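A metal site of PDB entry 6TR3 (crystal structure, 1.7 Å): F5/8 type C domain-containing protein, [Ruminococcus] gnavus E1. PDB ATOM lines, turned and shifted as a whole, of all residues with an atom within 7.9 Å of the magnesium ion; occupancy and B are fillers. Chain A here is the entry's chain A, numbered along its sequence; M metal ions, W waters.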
ATOM      1  N   LEU A 184      23.939  -3.021   3.971  1.00  0.00           N
ATOM      2  CA  LEU A 184      23.476  -3.378   5.309  1.00  0.00           C
ATOM      3  C   LEU A 184      22.280  -4.332   5.193  1.00  0.00           C
ATOM      4  O   LEU A 184      22.233  -5.377   5.844  1.00  0.00           O
ATOM      5  CB  LEU A 184      23.069  -2.150   6.103  1.00  0.00           C
ATOM      6  CG  LEU A 184      24.135  -1.246   6.702  1.00  0.00           C
ATOM      7  CD1 LEU A 184      23.443   0.006   7.227  1.00  0.00           C
ATOM      8  CD2 LEU A 184      24.926  -1.932   7.792  1.00  0.00           C
ATOM      9  N   GLU A 185      21.310  -3.968   4.346  1.00  0.00           N
ATOM     10  CA  GLU A 185      20.118  -4.795   4.146  1.00  0.00           C
ATOM     11  C   GLU A 185      20.494  -6.204   3.600  1.00  0.00           C
ATOM     12  O   GLU A 185      19.960  -7.208   4.036  1.00  0.00           O
ATOM     13  CB  GLU A 185      19.118  -4.060   3.242  1.00  0.00           C
ATOM     14  CG  GLU A 185      17.900  -4.887   2.834  1.00  0.00           C
ATOM     15  CD  GLU A 185      16.955  -5.217   3.977  1.00  0.00           C
ATOM     16  OE1 GLU A 185      17.015  -4.543   5.030  1.00  0.00           O
ATOM     17  OE2 GLU A 185      16.115  -6.128   3.813  1.00  0.00           O
ATOM     18  N   GLU A 186      21.440  -6.232   2.655  1.00  0.00           N
ATOM     19  CA  GLU A 186      21.874  -7.465   1.979  1.00  0.00           C
ATOM     20  C   GLU A 186      22.473  -8.452   2.981  1.00  0.00           C
ATOM     21  O   GLU A 186      22.184  -9.643   2.941  1.00  0.00           O
ATOM     22  CB  GLU A 186      22.878  -7.131   0.851  1.00  0.00           C
ATOM     23  CG  GLU A 186      23.275  -8.332   0.037  1.00  0.00           C
ATOM     24  CD  GLU A 186      24.246  -8.023  -1.048  1.00  0.00           C
ATOM     25  OE1 GLU A 186      25.210  -7.257  -0.789  1.00  0.00           O
ATOM     26  OE2 GLU A 186      24.042  -8.551  -2.173  1.00  0.00           O
ATOM     27  N   ILE A 187      23.306  -7.939   3.888  1.00  0.00           N
ATOM     28  CA  ILE A 187      23.929  -8.769   4.913  1.00  0.00           C
ATOM     29  C   ILE A 187      22.948  -9.103   6.050  1.00  0.00           C
ATOM     30  O   ILE A 187      22.772 -10.257   6.422  1.00  0.00           O
ATOM     31  CB  ILE A 187      25.163  -8.085   5.474  1.00  0.00           C
ATOM     32  CG1 ILE A 187      26.208  -7.916   4.357  1.00  0.00           C
ATOM     33  CG2 ILE A 187      25.724  -8.921   6.625  1.00  0.00           C
ATOM     34  CD1 ILE A 187      27.393  -7.107   4.748  1.00  0.00           C
ATOM     35  N   LEU A 188      22.321  -8.061   6.604  1.00  0.00           N
ATOM     36  CA  LEU A 188      21.535  -8.218   7.832  1.00  0.00           C
ATOM     37  C   LEU A 188      20.239  -8.953   7.568  1.00  0.00           C
ATOM     38  O   LEU A 188      19.704  -9.638   8.448  1.00  0.00           O
ATOM     39  CB  LEU A 188      21.291  -6.877   8.521  1.00  0.00           C
ATOM     40  CG  LEU A 188      22.580  -6.152   8.936  1.00  0.00           C
ATOM     41  CD1 LEU A 188      22.270  -4.803   9.589  1.00  0.00           C
ATOM     42  CD2 LEU A 188      23.456  -7.003   9.853  1.00  0.00           C
ATOM     43  N   GLY A 189      19.728  -8.808   6.340  1.00  0.00           N
ATOM     44  CA  GLY A 189      18.476  -9.416   5.939  1.00  0.00           C
ATOM     45  C   GLY A 189      18.581 -10.863   5.484  1.00  0.00           C
ATOM     46  O   GLY A 189      17.561 -11.506   5.307  1.00  0.00           O
ATOM     47  N   ASN A 190      19.802 -11.352   5.282  1.00  0.00           N
ATOM     48  CA  ASN A 190      20.003 -12.715   4.788  1.00  0.00           C
ATOM     49  C   ASN A 190      20.347 -13.690   5.908  1.00  0.00           C
ATOM     50  O   ASN A 190      21.309 -13.476   6.642  1.00  0.00           O
ATOM     51  CB  ASN A 190      21.101 -12.737   3.721  1.00  0.00           C
ATOM     52  CG  ASN A 190      21.145 -14.040   2.936  1.00  0.00           C
ATOM     53  OD1 ASN A 190      21.043 -15.140   3.512  1.00  0.00           O
ATOM     54  ND2 ASN A 190      21.313 -13.938   1.607  1.00  0.00           N
ATOM     55  N   PRO A 191      19.560 -14.785   6.105  1.00  0.00           N
ATOM     56  CA  PRO A 191      19.830 -15.725   7.191  1.00  0.00           C
ATOM     57  C   PRO A 191      21.234 -16.348   7.219  1.00  0.00           C
ATOM     58  O   PRO A 191      21.650 -16.814   8.272  1.00  0.00           O
ATOM     59  CB  PRO A 191      18.771 -16.821   6.988  1.00  0.00           C
ATOM     60  CG  PRO A 191      17.714 -16.224   6.111  1.00  0.00           C
ATOM     61  CD  PRO A 191      18.368 -15.135   5.302  1.00  0.00           C
ATOM     62  N   LYS A 192      21.947 -16.348   6.101  1.00  0.00           N
ATOM     63  CA  LYS A 192      23.245 -17.013   6.037  1.00  0.00           C
ATOM     64  C   LYS A 192      24.390 -16.202   6.662  1.00  0.00           C
ATOM     65  O   LYS A 192      25.483 -16.719   6.782  1.00  0.00           O
ATOM     66  CB  LYS A 192      23.587 -17.419   4.596  1.00  0.00           C
ATOM     67  CG  LYS A 192      24.167 -16.332   3.703  1.00  0.00           C
ATOM     68  CD  LYS A 192      24.112 -16.810   2.234  1.00  0.00           C
ATOM     69  CE  LYS A 192      24.528 -15.747   1.244  1.00  0.00           C
ATOM     70  NZ  LYS A 192      24.362 -16.277  -0.145  1.00  0.00           N
ATOM     71  N   TYR A 193      24.139 -14.945   7.043  1.00  0.00           N
ATOM     72  CA  TYR A 193      25.126 -14.120   7.709  1.00  0.00           C
ATOM     73  C   TYR A 193      24.735 -13.901   9.159  1.00  0.00           C
ATOM     74  O   TYR A 193      23.556 -13.629   9.453  1.00  0.00           O
ATOM     75  CB  TYR A 193      25.273 -12.759   7.013  1.00  0.00           C
ATOM     76  CG  TYR A 193      25.609 -12.839   5.545  1.00  0.00           C
ATOM     77  CD1 TYR A 193      26.799 -13.428   5.117  1.00  0.00           C
ATOM     78  CD2 TYR A 193      24.752 -12.303   4.584  1.00  0.00           C
ATOM     79  CE1 TYR A 193      27.113 -13.501   3.770  1.00  0.00           C
ATOM     80  CE2 TYR A 193      25.052 -12.358   3.228  1.00  0.00           C
ATOM     81  CZ  TYR A 193      26.230 -12.973   2.822  1.00  0.00           C
ATOM     82  OH  TYR A 193      26.514 -13.018   1.497  1.00  0.00           O
ATOM     83  N   GLY A 194      25.740 -13.979  10.047  1.00  0.00           N
ATOM     84  CA  GLY A 194      25.527 -13.827  11.484  1.00  0.00           C
ATOM     85  C   GLY A 194      25.454 -15.156  12.204  1.00  0.00           C
ATOM     86  O   GLY A 194      25.528 -16.219  11.572  1.00  0.00           O
ATOM     87  N   ASN A 195      25.273 -15.084  13.530  1.00  0.00           N
ATOM     88  CA  ASN A 195      24.952 -16.249  14.355  1.00  0.00           C
ATOM     89  C   ASN A 195      23.461 -16.542  14.226  1.00  0.00           C
ATOM     90  O   ASN A 195      22.642 -15.890  14.875  1.00  0.00           O
ATOM     91  CB  ASN A 195      25.325 -15.986  15.825  1.00  0.00           C
ATOM     92  CG  ASN A 195      25.102 -17.208  16.704  1.00  0.00           C
ATOM     93  OD1 ASN A 195      24.731 -18.262  16.227  1.00  0.00           O
ATOM     94  ND2 ASN A 195      25.293 -17.042  18.020  1.00  0.00           N
ATOM     95  N   ASP A 196      23.134 -17.528  13.382  1.00  0.00           N
ATOM     96  CA  ASP A 196      21.767 -17.862  13.053  1.00  0.00           C
ATOM     97  C   ASP A 196      21.031 -16.593  12.607  1.00  0.00           C
ATOM     98  O   ASP A 196      19.953 -16.280  13.104  1.00  0.00           O
ATOM     99  CB  ASP A 196      21.082 -18.508  14.265  1.00  0.00           C
ATOM    100  CG  ASP A 196      19.809 -19.249  13.899  1.00  0.00           C
ATOM    101  OD1 ASP A 196      19.652 -19.680  12.738  1.00  0.00           O
ATOM    102  OD2 ASP A 196      18.955 -19.392  14.811  1.00  0.00           O
ATOM    103  N   GLY A 197      21.652 -15.864  11.670  1.00  0.00           N
ATOM    104  CA  GLY A 197      21.083 -14.667  11.052  1.00  0.00           C
ATOM    105  C   GLY A 197      21.271 -13.369  11.819  1.00  0.00           C
ATOM    106  O   GLY A 197      20.909 -12.311  11.330  1.00  0.00           O
ATOM    107  N   HIS A 198      21.812 -13.452  13.034  1.00  0.00           N
ATOM    108  CA  HIS A 198      21.846 -12.324  13.957  1.00  0.00           C
ATOM    109  C   HIS A 198      23.227 -11.770  14.179  1.00  0.00           C
ATOM    110  O   HIS A 198      24.183 -12.526  14.385  1.00  0.00           O
ATOM    111  CB  HIS A 198      21.230 -12.716  15.308  1.00  0.00           C
ATOM    112  CG  HIS A 198      20.910 -11.550  16.187  1.00  0.00           C
ATOM    113  ND1 HIS A 198      21.150 -11.539  17.553  1.00  0.00           N
ATOM    114  CD2 HIS A 198      20.353 -10.349  15.890  1.00  0.00           C
ATOM    115  CE1 HIS A 198      20.743 -10.386  18.058  1.00  0.00           C
ATOM    116  NE2 HIS A 198      20.283  -9.636  17.062  1.00  0.00           N
ATOM    117  N   PHE A 199      23.325 -10.434  14.119  1.00  0.00           N
ATOM    118  CA  PHE A 199      24.467  -9.698  14.606  1.00  0.00           C
ATOM    119  C   PHE A 199      24.006  -8.899  15.815  1.00  0.00           C
ATOM    120  O   PHE A 199      22.892  -8.374  15.838  1.00  0.00           O
ATOM    121  CB  PHE A 199      25.003  -8.744  13.548  1.00  0.00           C
ATOM    122  CG  PHE A 199      25.652  -9.444  12.372  1.00  0.00           C
ATOM    123  CD1 PHE A 199      24.900  -9.886  11.296  1.00  0.00           C
ATOM    124  CD2 PHE A 199      27.012  -9.634  12.342  1.00  0.00           C
ATOM    125  CE1 PHE A 199      25.501 -10.512  10.212  1.00  0.00           C
ATOM    126  CE2 PHE A 199      27.624 -10.286  11.278  1.00  0.00           C
ATOM    127  CZ  PHE A 199      26.863 -10.701  10.192  1.00  0.00           C
ATOM    128  N   ILE A 226      19.399  -1.368  10.228  1.00  0.00           N
ATOM    129  CA  ILE A 226      20.019  -2.266  11.206  1.00  0.00           C
ATOM    130  C   ILE A 226      18.974  -2.815  12.162  1.00  0.00           C
ATOM    131  O   ILE A 226      18.902  -4.031  12.377  1.00  0.00           O
ATOM    132  CB  ILE A 226      21.165  -1.582  11.974  1.00  0.00           C
ATOM    133  CG1 ILE A 226      22.335  -1.297  11.015  1.00  0.00           C
ATOM    134  CG2 ILE A 226      21.646  -2.467  13.132  1.00  0.00           C
ATOM    135  CD1 ILE A 226      23.357  -0.341  11.565  1.00  0.00           C
ATOM    136  N   ASN A 229      16.296  -5.333  11.013  1.00  0.00           N
ATOM    137  CA  ASN A 229      16.829  -6.675  10.814  1.00  0.00           C
ATOM    138  C   ASN A 229      17.389  -7.370  12.052  1.00  0.00           C
ATOM    139  O   ASN A 229      17.383  -8.594  12.132  1.00  0.00           O
ATOM    140  CB  ASN A 229      17.914  -6.612   9.746  1.00  0.00           C
ATOM    141  CG  ASN A 229      17.333  -6.453   8.362  1.00  0.00           C
ATOM    142  OD1 ASN A 229      16.704  -7.369   7.851  1.00  0.00           O
ATOM    143  ND2 ASN A 229      17.489  -5.268   7.780  1.00  0.00           N
ATOM    144  N   GLU A 230      17.910  -6.566  12.976  1.00  0.00           N
ATOM    145  CA  GLU A 230      18.677  -7.080  14.103  1.00  0.00           C
ATOM    146  C   GLU A 230      18.313  -6.487  15.481  1.00  0.00           C
ATOM    147  O   GLU A 230      18.992  -6.800  16.460  1.00  0.00           O
ATOM    148  CB  GLU A 230      20.173  -6.859  13.843  1.00  0.00           C
ATOM    149  CG  GLU A 230      20.686  -7.314  12.470  1.00  0.00           C
ATOM    150  CD  GLU A 230      20.670  -8.831  12.257  1.00  0.00           C
ATOM    151  OE1 GLU A 230      20.546  -9.558  13.237  1.00  0.00           O
ATOM    152  OE2 GLU A 230      20.786  -9.320  11.096  1.00  0.00           O
ATOM    153  N   ALA A 234      12.788  -6.157  14.723  1.00  0.00           N
ATOM    154  CA  ALA A 234      12.944  -7.513  14.172  1.00  0.00           C
ATOM    155  C   ALA A 234      12.536  -8.625  15.143  1.00  0.00           C
ATOM    156  O   ALA A 234      12.582  -9.801  14.787  1.00  0.00           O
ATOM    157  CB  ALA A 234      14.386  -7.735  13.736  1.00  0.00           C
ATOM    158  N   TYR A 236      13.879  -9.003  18.410  1.00  0.00           N
ATOM    159  CA  TYR A 236      14.916  -9.257  19.420  1.00  0.00           C
ATOM    160  C   TYR A 236      14.608  -8.452  20.698  1.00  0.00           C
ATOM    161  O   TYR A 236      13.842  -7.499  20.684  1.00  0.00           O
ATOM    162  CB  TYR A 236      16.321  -8.932  18.843  1.00  0.00           C
ATOM    163  CG  TYR A 236      16.709  -9.890  17.733  1.00  0.00           C
ATOM    164  CD1 TYR A 236      17.208 -11.163  18.016  1.00  0.00           C
ATOM    165  CD2 TYR A 236      16.550  -9.546  16.402  1.00  0.00           C
ATOM    166  CE1 TYR A 236      17.524 -12.055  17.020  1.00  0.00           C
ATOM    167  CE2 TYR A 236      16.860 -10.425  15.387  1.00  0.00           C
ATOM    168  CZ  TYR A 236      17.344 -11.688  15.711  1.00  0.00           C
ATOM    169  OH  TYR A 236      17.681 -12.581  14.694  1.00  0.00           O
HETATM  170 MG    MG M   1      20.247 -10.979   9.964  1.00  0.00          MG
HETATM  171  O   HOH W   1      22.134 -11.195   9.072  1.00  0.00           O
HETATM  172  O   HOH W   2      18.395 -10.775  10.783  1.00  0.00           O
HETATM  173  O   HOH W   3      19.629 -12.568   8.806  1.00  0.00           O
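O of Glu 230 lies within hydrogen-bond range of NE2 of His 198, at 3.2 Å. The side-chain carboxylate (OE1) of Glu 230 is in hydrogen-bond range of the backbone NH (N) of Phe 199.
The nearest printed residue that does not touch the magnesium ion is His 198 (4.2 Å).
The magnesium ion is bound by the backbone carbonyl oxygen of Gly 197 (2.0 Å), water W2 (2.0 Å), water W3 (2.1 Å), the side-chain carboxylate of Glu 230 (2.1 Å), the backbone carbonyl oxygen of Leu 188 (2.1 Å) and water W1 (2.1 Å).
Water W2 lies within hydrogen-bond range of the backbone carbonyl oxygen (O) of Asn 229 (2.8 Å) and the side-chain carboxylate (OE1) of Glu 230 (3.5 Å).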
